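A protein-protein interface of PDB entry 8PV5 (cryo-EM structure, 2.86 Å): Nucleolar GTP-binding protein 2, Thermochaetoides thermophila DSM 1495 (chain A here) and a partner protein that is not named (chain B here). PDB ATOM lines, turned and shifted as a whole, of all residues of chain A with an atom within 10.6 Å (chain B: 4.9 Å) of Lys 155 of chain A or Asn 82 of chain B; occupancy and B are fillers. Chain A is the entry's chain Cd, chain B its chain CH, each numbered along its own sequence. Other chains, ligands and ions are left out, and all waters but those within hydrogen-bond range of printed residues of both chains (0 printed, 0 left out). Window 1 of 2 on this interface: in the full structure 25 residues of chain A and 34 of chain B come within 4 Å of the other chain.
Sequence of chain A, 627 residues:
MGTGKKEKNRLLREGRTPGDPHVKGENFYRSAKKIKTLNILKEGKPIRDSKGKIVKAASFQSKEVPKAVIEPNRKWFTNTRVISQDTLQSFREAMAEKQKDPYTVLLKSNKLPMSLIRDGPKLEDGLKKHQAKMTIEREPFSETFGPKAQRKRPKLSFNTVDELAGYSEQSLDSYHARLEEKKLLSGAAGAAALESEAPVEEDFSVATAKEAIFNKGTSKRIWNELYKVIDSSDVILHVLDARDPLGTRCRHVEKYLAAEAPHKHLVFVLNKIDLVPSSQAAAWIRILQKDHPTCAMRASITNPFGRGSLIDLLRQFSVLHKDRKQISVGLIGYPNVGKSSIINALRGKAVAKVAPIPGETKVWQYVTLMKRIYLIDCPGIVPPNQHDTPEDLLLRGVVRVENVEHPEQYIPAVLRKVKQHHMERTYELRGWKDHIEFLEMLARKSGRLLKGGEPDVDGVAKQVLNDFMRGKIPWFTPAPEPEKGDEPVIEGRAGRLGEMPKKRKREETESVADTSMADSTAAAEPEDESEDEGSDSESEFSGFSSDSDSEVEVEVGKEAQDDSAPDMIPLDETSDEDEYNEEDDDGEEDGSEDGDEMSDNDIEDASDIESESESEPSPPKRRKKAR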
ATOM      1  N   GLN A 131      -2.255 -11.199  -6.960  1.00  0.00           N
ATOM      2  CA  GLN A 131      -3.200 -10.168  -6.516  1.00  0.00           C
ATOM      3  C   GLN A 131      -4.640 -10.503  -6.895  1.00  0.00           C
ATOM      4  O   GLN A 131      -5.560 -10.305  -6.091  1.00  0.00           O
ATOM      5  CB  GLN A 131      -2.821  -8.805  -7.101  1.00  0.00           C
ATOM      6  CG  GLN A 131      -1.747  -8.052  -6.341  1.00  0.00           C
ATOM      7  CD  GLN A 131      -2.169  -7.696  -4.932  1.00  0.00           C
ATOM      8  OE1 GLN A 131      -1.675  -8.268  -3.961  1.00  0.00           O
ATOM      9  NE2 GLN A 131      -3.089  -6.749  -4.813  1.00  0.00           N
ATOM     10  N   MET A 134      -5.928 -13.304  -4.674  1.00  0.00           N
ATOM     11  CA  MET A 134      -6.172 -12.754  -3.341  1.00  0.00           C
ATOM     12  C   MET A 134      -7.472 -11.968  -3.289  1.00  0.00           C
ATOM     13  O   MET A 134      -8.218 -12.077  -2.314  1.00  0.00           O
ATOM     14  CB  MET A 134      -5.025 -11.846  -2.908  1.00  0.00           C
ATOM     15  CG  MET A 134      -3.711 -12.527  -2.665  1.00  0.00           C
ATOM     16  SD  MET A 134      -2.479 -11.315  -2.181  1.00  0.00           S
ATOM     17  CE  MET A 134      -1.051 -12.368  -2.074  1.00  0.00           C
ATOM     18  N   THR A 135      -7.745 -11.150  -4.311  1.00  0.00           N
ATOM     19  CA  THR A 135      -8.987 -10.378  -4.323  1.00  0.00           C
ATOM     20  C   THR A 135     -10.205 -11.289  -4.411  1.00  0.00           C
ATOM     21  O   THR A 135     -11.221 -11.048  -3.741  1.00  0.00           O
ATOM     22  CB  THR A 135      -8.988  -9.376  -5.477  1.00  0.00           C
ATOM     23  OG1 THR A 135      -8.683 -10.049  -6.704  1.00  0.00           O
ATOM     24  CG2 THR A 135      -7.969  -8.272  -5.235  1.00  0.00           C
ATOM     25  N   ARG A 138     -10.663 -12.851  -1.087  1.00  0.00           N
ATOM     26  CA  ARG A 138     -11.048 -11.869  -0.082  1.00  0.00           C
ATOM     27  C   ARG A 138     -12.528 -11.532  -0.185  1.00  0.00           C
ATOM     28  O   ARG A 138     -13.224 -11.462   0.835  1.00  0.00           O
ATOM     29  CB  ARG A 138     -10.190 -10.614  -0.224  1.00  0.00           C
ATOM     30  CG  ARG A 138     -10.376  -9.611   0.895  1.00  0.00           C
ATOM     31  CD  ARG A 138      -9.749  -8.263   0.566  1.00  0.00           C
ATOM     32  NE  ARG A 138      -8.434  -8.388  -0.052  1.00  0.00           N
ATOM     33  CZ  ARG A 138      -8.152  -8.026  -1.296  1.00  0.00           C
ATOM     34  NH1 ARG A 138      -9.070  -7.500  -2.088  1.00  0.00           N
ATOM     35  NH2 ARG A 138      -6.916  -8.195  -1.755  1.00  0.00           N
ATOM     36  N   GLU A 139     -13.031 -11.322  -1.399  1.00  0.00           N
ATOM     37  CA  GLU A 139     -14.474 -11.283  -1.627  1.00  0.00           C
ATOM     38  C   GLU A 139     -14.792 -11.896  -2.986  1.00  0.00           C
ATOM     39  O   GLU A 139     -14.161 -11.547  -4.000  1.00  0.00           O
ATOM     40  CB  GLU A 139     -15.044  -9.870  -1.479  1.00  0.00           C
ATOM     41  CG  GLU A 139     -14.613  -8.816  -2.487  1.00  0.00           C
ATOM     42  CD  GLU A 139     -13.343  -8.085  -2.095  1.00  0.00           C
ATOM     43  OE1 GLU A 139     -12.625  -8.567  -1.200  1.00  0.00           O
ATOM     44  OE2 GLU A 139     -13.064  -7.020  -2.683  1.00  0.00           O
ATOM     45  N   THR A 144     -19.907  -9.319  -4.490  1.00  0.00           N
ATOM     46  CA  THR A 144     -19.635  -7.981  -5.004  1.00  0.00           C
ATOM     47  C   THR A 144     -20.850  -7.391  -5.705  1.00  0.00           C
ATOM     48  O   THR A 144     -21.318  -6.304  -5.344  1.00  0.00           O
ATOM     49  CB  THR A 144     -18.446  -8.021  -5.959  1.00  0.00           C
ATOM     50  OG1 THR A 144     -17.297  -8.533  -5.274  1.00  0.00           O
ATOM     51  CG2 THR A 144     -18.155  -6.639  -6.489  1.00  0.00           C
ATOM     52  N   PHE A 145     -21.375  -8.089  -6.708  1.00  0.00           N
ATOM     53  CA  PHE A 145     -22.486  -7.580  -7.494  1.00  0.00           C
ATOM     54  C   PHE A 145     -23.431  -8.726  -7.809  1.00  0.00           C
ATOM     55  O   PHE A 145     -23.004  -9.868  -7.997  1.00  0.00           O
ATOM     56  CB  PHE A 145     -21.996  -6.919  -8.787  1.00  0.00           C
ATOM     57  CG  PHE A 145     -23.027  -6.060  -9.455  1.00  0.00           C
ATOM     58  CD1 PHE A 145     -23.291  -4.784  -8.989  1.00  0.00           C
ATOM     59  CD2 PHE A 145     -23.736  -6.531 -10.547  1.00  0.00           C
ATOM     60  CE1 PHE A 145     -24.241  -3.992  -9.602  1.00  0.00           C
ATOM     61  CE2 PHE A 145     -24.687  -5.744 -11.163  1.00  0.00           C
ATOM     62  CZ  PHE A 145     -24.941  -4.476 -10.689  1.00  0.00           C
ATOM     63  N   ARG A 151     -21.752  -6.207  -0.829  1.00  0.00           N
ATOM     64  CA  ARG A 151     -20.792  -5.114  -0.812  1.00  0.00           C
ATOM     65  C   ARG A 151     -21.502  -3.784  -0.595  1.00  0.00           C
ATOM     66  O   ARG A 151     -22.443  -3.437  -1.312  1.00  0.00           O
ATOM     67  CB  ARG A 151     -20.007  -5.095  -2.123  1.00  0.00           C
ATOM     68  CG  ARG A 151     -19.207  -3.834  -2.381  1.00  0.00           C
ATOM     69  CD  ARG A 151     -18.413  -3.973  -3.669  1.00  0.00           C
ATOM     70  NE  ARG A 151     -17.701  -2.754  -4.027  1.00  0.00           N
ATOM     71  CZ  ARG A 151     -18.134  -1.869  -4.913  1.00  0.00           C
ATOM     72  NH1 ARG A 151     -19.290  -2.024  -5.535  1.00  0.00           N
ATOM     73  NH2 ARG A 151     -17.389  -0.801  -5.182  1.00  0.00           N
ATOM     74  N   LYS A 152     -21.048  -3.045   0.403  1.00  0.00           N
ATOM     75  CA  LYS A 152     -21.603  -1.735   0.720  1.00  0.00           C
ATOM     76  C   LYS A 152     -20.566  -0.626   0.663  1.00  0.00           C
ATOM     77  O   LYS A 152     -20.867   0.460   0.166  1.00  0.00           O
ATOM     78  CB  LYS A 152     -22.259  -1.762   2.109  1.00  0.00           C
ATOM     79  CG  LYS A 152     -23.659  -2.351   2.121  1.00  0.00           C
ATOM     80  CD  LYS A 152     -24.681  -1.340   1.633  1.00  0.00           C
ATOM     81  CE  LYS A 152     -26.094  -1.876   1.754  1.00  0.00           C
ATOM     82  NZ  LYS A 152     -27.097  -0.886   1.275  1.00  0.00           N
ATOM     83  N   ARG A 153     -19.354  -0.874   1.148  1.00  0.00           N
ATOM     84  CA  ARG A 153     -18.302   0.132   1.117  1.00  0.00           C
ATOM     85  C   ARG A 153     -17.423  -0.069  -0.104  1.00  0.00           C
ATOM     86  O   ARG A 153     -16.806  -1.135  -0.245  1.00  0.00           O
ATOM     87  CB  ARG A 153     -17.452   0.061   2.380  1.00  0.00           C
ATOM     88  CG  ARG A 153     -18.209   0.382   3.656  1.00  0.00           C
ATOM     89  CD  ARG A 153     -18.591   1.848   3.707  1.00  0.00           C
ATOM     90  NE  ARG A 153     -19.221   2.205   4.972  1.00  0.00           N
ATOM     91  CZ  ARG A 153     -20.527   2.165   5.194  1.00  0.00           C
ATOM     92  NH1 ARG A 153     -21.376   1.782   4.256  1.00  0.00           N
ATOM     93  NH2 ARG A 153     -20.992   2.518   6.389  1.00  0.00           N
ATOM     94  N   PRO A 154     -17.340   0.906  -1.002  1.00  0.00           N
ATOM     95  CA  PRO A 154     -16.481   0.767  -2.180  1.00  0.00           C
ATOM     96  C   PRO A 154     -15.010   0.925  -1.815  1.00  0.00           C
ATOM     97  O   PRO A 154     -14.650   1.439  -0.756  1.00  0.00           O
ATOM     98  CB  PRO A 154     -16.951   1.903  -3.091  1.00  0.00           C
ATOM     99  CG  PRO A 154     -17.440   2.940  -2.149  1.00  0.00           C
ATOM    100  CD  PRO A 154     -18.032   2.206  -0.973  1.00  0.00           C
ATOM    101  N   LYS A 155     -14.157   0.467  -2.726  1.00  0.00           N
ATOM    102  CA  LYS A 155     -12.713   0.593  -2.585  1.00  0.00           C
ATOM    103  C   LYS A 155     -12.270   1.886  -3.257  1.00  0.00           C
ATOM    104  O   LYS A 155     -12.563   2.108  -4.436  1.00  0.00           O
ATOM    105  CB  LYS A 155     -11.991  -0.605  -3.196  1.00  0.00           C
ATOM    106  CG  LYS A 155     -10.483  -0.562  -3.024  1.00  0.00           C
ATOM    107  CD  LYS A 155      -9.816  -1.780  -3.635  1.00  0.00           C
ATOM    108  CE  LYS A 155      -8.318  -1.767  -3.382  1.00  0.00           C
ATOM    109  NZ  LYS A 155      -7.647  -0.650  -4.102  1.00  0.00           N
ATOM    110  N   LEU A 156     -11.567   2.729  -2.509  1.00  0.00           N
ATOM    111  CA  LEU A 156     -11.186   4.053  -2.970  1.00  0.00           C
ATOM    112  C   LEU A 156      -9.674   4.218  -2.912  1.00  0.00           C
ATOM    113  O   LEU A 156      -8.994   3.633  -2.065  1.00  0.00           O
ATOM    114  CB  LEU A 156     -11.859   5.143  -2.128  1.00  0.00           C
ATOM    115  CG  LEU A 156     -13.365   4.993  -1.915  1.00  0.00           C
ATOM    116  CD1 LEU A 156     -13.866   6.043  -0.943  1.00  0.00           C
ATOM    117  CD2 LEU A 156     -14.104   5.079  -3.237  1.00  0.00           C
ATOM    118  N   SER A 157      -9.156   5.029  -3.831  1.00  0.00           N
ATOM    119  CA  SER A 157      -7.744   5.380  -3.864  1.00  0.00           C
ATOM    120  C   SER A 157      -7.473   6.734  -3.224  1.00  0.00           C
ATOM    121  O   SER A 157      -6.363   7.260  -3.354  1.00  0.00           O
ATOM    122  CB  SER A 157      -7.231   5.372  -5.304  1.00  0.00           C
ATOM    123  OG  SER A 157      -7.746   6.471  -6.032  1.00  0.00           O
ATOM    124  N   PHE A 158      -8.461   7.308  -2.542  1.00  0.00           N
ATOM    125  CA  PHE A 158      -8.332   8.626  -1.941  1.00  0.00           C
ATOM    126  C   PHE A 158      -8.835   8.573  -0.506  1.00  0.00           C
ATOM    127  O   PHE A 158      -9.682   7.751  -0.149  1.00  0.00           O
ATOM    128  CB  PHE A 158      -9.091   9.692  -2.746  1.00  0.00           C
ATOM    129  CG  PHE A 158     -10.396   9.210  -3.316  1.00  0.00           C
ATOM    130  CD1 PHE A 158     -11.555   9.256  -2.561  1.00  0.00           C
ATOM    131  CD2 PHE A 158     -10.465   8.723  -4.612  1.00  0.00           C
ATOM    132  CE1 PHE A 158     -12.756   8.815  -3.084  1.00  0.00           C
ATOM    133  CE2 PHE A 158     -11.662   8.280  -5.139  1.00  0.00           C
ATOM    134  CZ  PHE A 158     -12.809   8.325  -4.373  1.00  0.00           C
ATOM    135  N   ASN A 159      -8.297   9.473   0.316  1.00  0.00           N
ATOM    136  CA  ASN A 159      -8.590   9.517   1.740  1.00  0.00           C
ATOM    137  C   ASN A 159      -9.477  10.694   2.123  1.00  0.00           C
ATOM    138  O   ASN A 159     -10.462  10.494   2.842  1.00  0.00           O
ATOM    139  CB  ASN A 159      -7.271   9.574   2.536  1.00  0.00           C
ATOM    140  CG  ASN A 159      -7.449   9.407   4.047  1.00  0.00           C
ATOM    141  OD1 ASN A 159      -8.553   9.268   4.563  1.00  0.00           O
ATOM    142  ND2 ASN A 159      -6.330   9.425   4.761  1.00  0.00           N
ATOM    143  N   LEU A 164      -9.399  13.747  -3.049  1.00  0.00           N
ATOM    144  CA  LEU A 164     -10.344  13.387  -4.103  1.00  0.00           C
ATOM    145  C   LEU A 164     -10.369  14.437  -5.208  1.00  0.00           C
ATOM    146  O   LEU A 164     -10.424  14.096  -6.396  1.00  0.00           O
ATOM    147  CB  LEU A 164     -11.740  13.198  -3.514  1.00  0.00           C
ATOM    148  CG  LEU A 164     -12.895  12.965  -4.491  1.00  0.00           C
ATOM    149  CD1 LEU A 164     -12.634  11.775  -5.399  1.00  0.00           C
ATOM    150  CD2 LEU A 164     -14.187  12.779  -3.729  1.00  0.00           C
ATOM    151  N   TYR A 167      -7.196  14.071  -7.160  1.00  0.00           N
ATOM    152  CA  TYR A 167      -7.306  12.866  -7.971  1.00  0.00           C
ATOM    153  C   TYR A 167      -8.167  13.107  -9.203  1.00  0.00           C
ATOM    154  O   TYR A 167      -7.841  12.630 -10.295  1.00  0.00           O
ATOM    155  CB  TYR A 167      -7.875  11.726  -7.126  1.00  0.00           C
ATOM    156  CG  TYR A 167      -8.379  10.541  -7.915  1.00  0.00           C
ATOM    157  CD1 TYR A 167      -7.495   9.661  -8.525  1.00  0.00           C
ATOM    158  CD2 TYR A 167      -9.741  10.291  -8.035  1.00  0.00           C
ATOM    159  CE1 TYR A 167      -7.953   8.572  -9.243  1.00  0.00           C
ATOM    160  CE2 TYR A 167     -10.208   9.207  -8.751  1.00  0.00           C
ATOM    161  CZ  TYR A 167      -9.311   8.351  -9.351  1.00  0.00           C
ATOM    162  OH  TYR A 167      -9.774   7.269 -10.063  1.00  0.00           O
ATOM    163  N   SER A 171      -6.705  12.895 -12.923  1.00  0.00           N
ATOM    164  CA  SER A 171      -7.361  11.941 -13.809  1.00  0.00           C
ATOM    165  C   SER A 171      -7.829  12.617 -15.089  1.00  0.00           C
ATOM    166  O   SER A 171      -7.693  12.059 -16.183  1.00  0.00           O
ATOM    167  CB  SER A 171      -8.535  11.279 -13.089  1.00  0.00           C
ATOM    168  OG  SER A 171      -8.085  10.473 -12.016  1.00  0.00           O
ATOM    169  N   ARG B  78     -15.398   6.161 -15.574  1.00  0.00           N
ATOM    170  CA  ARG B  78     -14.523   5.147 -14.990  1.00  0.00           C
ATOM    171  C   ARG B  78     -14.733   5.028 -13.486  1.00  0.00           C
ATOM    172  O   ARG B  78     -14.859   3.920 -12.952  1.00  0.00           O
ATOM    173  CB  ARG B  78     -13.066   5.485 -15.299  1.00  0.00           C
ATOM    174  CG  ARG B  78     -12.053   4.572 -14.636  1.00  0.00           C
ATOM    175  CD  ARG B  78     -10.645   5.107 -14.815  1.00  0.00           C
ATOM    176  NE  ARG B  78     -10.425   5.621 -16.161  1.00  0.00           N
ATOM    177  CZ  ARG B  78      -9.718   6.707 -16.444  1.00  0.00           C
ATOM    178  NH1 ARG B  78      -9.146   7.427 -15.492  1.00  0.00           N
ATOM    179  NH2 ARG B  78      -9.582   7.081 -17.713  1.00  0.00           N
ATOM    180  N   ASP B  79     -14.813   6.160 -12.788  1.00  0.00           N
ATOM    181  CA  ASP B  79     -14.987   6.105 -11.343  1.00  0.00           C
ATOM    182  C   ASP B  79     -16.415   5.727 -10.965  1.00  0.00           C
ATOM    183  O   ASP B  79     -16.638   5.113  -9.918  1.00  0.00           O
ATOM    184  CB  ASP B  79     -14.567   7.437 -10.730  1.00  0.00           C
ATOM    185  CG  ASP B  79     -13.070   7.664 -10.834  1.00  0.00           C
ATOM    186  OD1 ASP B  79     -12.323   6.665 -10.839  1.00  0.00           O
ATOM    187  OD2 ASP B  79     -12.635   8.827 -10.938  1.00  0.00           O
ATOM    188  N   LEU B  80     -17.391   6.042 -11.819  1.00  0.00           N
ATOM    189  CA  LEU B  80     -18.755   5.579 -11.588  1.00  0.00           C
ATOM    190  C   LEU B  80     -18.845   4.066 -11.720  1.00  0.00           C
ATOM    191  O   LEU B  80     -19.542   3.405 -10.943  1.00  0.00           O
ATOM    192  CB  LEU B  80     -19.714   6.260 -12.563  1.00  0.00           C
ATOM    193  CG  LEU B  80     -21.197   5.962 -12.337  1.00  0.00           C
ATOM    194  CD1 LEU B  80     -21.606   6.339 -10.925  1.00  0.00           C
ATOM    195  CD2 LEU B  80     -22.053   6.687 -13.361  1.00  0.00           C
ATOM    196  N   MET B  81     -18.144   3.498 -12.702  1.00  0.00           N
ATOM    197  CA  MET B  81     -18.089   2.045 -12.815  1.00  0.00           C
ATOM    198  C   MET B  81     -17.311   1.436 -11.655  1.00  0.00           C
ATOM    199  O   MET B  81     -17.608   0.319 -11.222  1.00  0.00           O
ATOM    200  CB  MET B  81     -17.478   1.642 -14.157  1.00  0.00           C
ATOM    201  CG  MET B  81     -18.346   1.996 -15.353  1.00  0.00           C
ATOM    202  SD  MET B  81     -17.616   1.527 -16.931  1.00  0.00           S
ATOM    203  CE  MET B  81     -18.835   2.173 -18.070  1.00  0.00           C
ATOM    204  N   ASN B  82     -16.319   2.163 -11.132  1.00  0.00           N
ATOM    205  CA  ASN B  82     -15.586   1.698  -9.955  1.00  0.00           C
ATOM    206  C   ASN B  82     -16.461   1.719  -8.703  1.00  0.00           C
ATOM    207  O   ASN B  82     -16.261   0.920  -7.780  1.00  0.00           O
ATOM    208  CB  ASN B  82     -14.335   2.557  -9.756  1.00  0.00           C
ATOM    209  CG  ASN B  82     -13.702   2.366  -8.395  1.00  0.00           C
ATOM    210  OD1 ASN B  82     -13.207   1.287  -8.074  1.00  0.00           O
ATOM    211  ND2 ASN B  82     -13.721   3.414  -7.582  1.00  0.00           N
ATOM    212  N   ILE B  83     -17.422   2.640  -8.638  1.00  0.00           N
ATOM    213  CA  ILE B  83     -18.332   2.663  -7.494  1.00  0.00           C
ATOM    214  C   ILE B  83     -19.406   1.591  -7.643  1.00  0.00           C
ATOM    215  O   ILE B  83     -19.704   0.856  -6.692  1.00  0.00           O
ATOM    216  CB  ILE B  83     -18.943   4.066  -7.315  1.00  0.00           C
ATOM    217  CG1 ILE B  83     -17.855   5.075  -6.950  1.00  0.00           C
ATOM    218  CG2 ILE B  83     -20.016   4.058  -6.245  1.00  0.00           C
ATOM    219  CD1 ILE B  83     -17.148   4.768  -5.652  1.00  0.00           C
ATOM    220  N   LEU B  84     -19.994   1.475  -8.837  1.00  0.00           N
ATOM    221  CA  LEU B  84     -21.083   0.523  -9.046  1.00  0.00           C
ATOM    222  C   LEU B  84     -20.592  -0.918  -8.996  1.00  0.00           C
ATOM    223  O   LEU B  84     -21.299  -1.801  -8.498  1.00  0.00           O
ATOM    224  CB  LEU B  84     -21.772   0.795 -10.382  1.00  0.00           C
ATOM    225  CG  LEU B  84     -22.546   2.103 -10.528  1.00  0.00           C
ATOM    226  CD1 LEU B  84     -23.017   2.278 -11.961  1.00  0.00           C
ATOM    227  CD2 LEU B  84     -23.718   2.135  -9.568  1.00  0.00           C
ATOM    228  N   TYR B  85     -19.392  -1.177  -9.504  1.00  0.00           N
ATOM    229  CA  TYR B  85     -18.849  -2.524  -9.587  1.00  0.00           C
ATOM    230  C   TYR B  85     -17.438  -2.438  -9.038  1.00  0.00           C
ATOM    231  O   TYR B  85     -16.798  -1.395  -9.167  1.00  0.00           O
ATOM    232  CB  TYR B  85     -18.795  -3.006 -11.035  1.00  0.00           C
ATOM    233  CG  TYR B  85     -20.028  -2.674 -11.832  1.00  0.00           C
ATOM    234  CD1 TYR B  85     -21.214  -3.372 -11.673  1.00  0.00           C
ATOM    235  CD2 TYR B  85     -19.994  -1.638 -12.754  1.00  0.00           C
ATOM    236  CE1 TYR B  85     -22.332  -3.039 -12.418  1.00  0.00           C
ATOM    237  CE2 TYR B  85     -21.095  -1.302 -13.494  1.00  0.00           C
ATOM    238  CZ  TYR B  85     -22.259  -2.001 -13.326  1.00  0.00           C
ATOM    239  OH  TYR B  85     -23.348  -1.644 -14.080  1.00  0.00           O
ATOM    240  N   ASP B  86     -16.938  -3.513  -8.444  1.00  0.00           N
ATOM    241  CA  ASP B  86     -15.530  -3.499  -8.079  1.00  0.00           C
ATOM    242  C   ASP B  86     -14.690  -3.544  -9.349  1.00  0.00           C
ATOM    243  O   ASP B  86     -14.821  -4.463 -10.162  1.00  0.00           O
ATOM    244  CB  ASP B  86     -15.192  -4.668  -7.160  1.00  0.00           C
ATOM    245  CG  ASP B  86     -13.869  -4.487  -6.453  1.00  0.00           C
ATOM    246  OD1 ASP B  86     -13.767  -3.579  -5.604  1.00  0.00           O
ATOM    247  OD2 ASP B  86     -12.935  -5.260  -6.733  1.00  0.00           O
ATOM    248  N   ALA B  87     -13.868  -2.508  -9.543  1.00  0.00           N
ATOM    249  CA  ALA B  87     -13.067  -2.404 -10.760  1.00  0.00           C
ATOM    250  C   ALA B  87     -12.053  -3.536 -10.848  1.00  0.00           C
ATOM    251  O   ALA B  87     -11.768  -4.044 -11.941  1.00  0.00           O
ATOM    252  CB  ALA B  87     -12.366  -1.049 -10.814  1.00  0.00           C
ATOM    253  N   ASP B  88     -11.513  -3.951  -9.699  1.00  0.00           N
ATOM    254  CA  ASP B  88     -10.640  -5.115  -9.663  1.00  0.00           C
ATOM    255  C   ASP B  88     -11.376  -6.369 -10.114  1.00  0.00           C
ATOM    256  O   ASP B  88     -10.844  -7.143 -10.909  1.00  0.00           O
ATOM    257  CB  ASP B  88     -10.067  -5.307  -8.259  1.00  0.00           C
ATOM    258  CG  ASP B  88      -9.083  -4.221  -7.879  1.00  0.00           C
ATOM    259  OD1 ASP B  88      -8.436  -3.656  -8.785  1.00  0.00           O
ATOM    260  OD2 ASP B  88      -8.955  -3.932  -6.672  1.00  0.00           O
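The guanidinium group of Arg 151 of chain A is in hydrogen-bond range of the backbone carbonyl oxygen of Asn 82 of chain B (3.3 Å). The guanidinium group of Arg 151 of chain A lies within hydrogen-bond range of the backbone carbonyl oxygen of Ile 83 of chain B, at 3.1 Å. OH of Tyr 167 of chain A lies within hydrogen-bond range of OD1 of Asp 79 of chain B (2.7 Å).
O of Tyr 167 of chain A is in hydrogen-bond range of OG of Ser 171 of chain A (2.8 Å).
Among the printed residues, merely in contact across the chains: Thr 144 of chain A with Asp 86 of chain B (3.6 Å), Phe 145 of chain A with Leu 84 of chain B (3.6 Å), Phe 145 of chain A with Tyr 85 of chain B (3.4 Å), Arg 151 of chain A with Leu 84 of chain B (3.6 Å), Arg 151 of chain A with Tyr 85 of chain B (3.98 Å), Pro 154 of chain A with Ile 83 of chain B (3.8 Å), Lys 155 of chain A with Asn 82 of chain B (3.6 Å), Lys 155 of chain A with Asp 88 of chain B (3.8 Å) and Leu 156 of chain A with Ile 83 of chain B (3.9 Å).
Lys 155 of chain A touches two residues of chain B. Of chain A, only Arg 151 (3.3 Å) and Lys 155 (3.6 Å) come within 4 Å of Asn 82 of chain B. Of chain A, only Thr 144 comes within 4 Å of Asp 86 of chain B. Of the printed residues of chain B, Phe 145 of chain A touches Leu 84 and Tyr 85. Of the printed residues of chain B, Arg 151 of chain A touches Asn 82, Ile 83, Leu 84 and Tyr 85. Printed residues of chain B within 4 Å of Leu 156 of chain A: Ile 83. Of the printed residues of chain A, Tyr 85 of chain B touches Phe 145 (3.4 Å) and Arg 151 (3.98 Å). Printed residues of chain A within 4 Å of Asp 88 of chain B: Lys 155 (3.8 Å). Arg 153 of chain A touches none of the printed residues of chain B. Ser 157 of chain A touches none of the printed residues of chain B. The nearest residue of chain B that does not touch Lys 155 of chain A is Asp 86 of chain B (4.2 Å). The nearest residue of chain A that does not touch Asn 82 of chain B is Leu 156 of chain A (4.7 Å).
Hydrophobic or aromatic side chains of chain B within 4 Å of the printed part of chain A: Ile 83 and Tyr 85. Of the 19 printed residues of chain A, 7 touch a printed residue of chain B. Printed residues of chain A that touch a printed residue of chain B: Thr 144, Phe 145, Arg 151, Pro 154, Lys 155, Leu 156 and Tyr 167.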
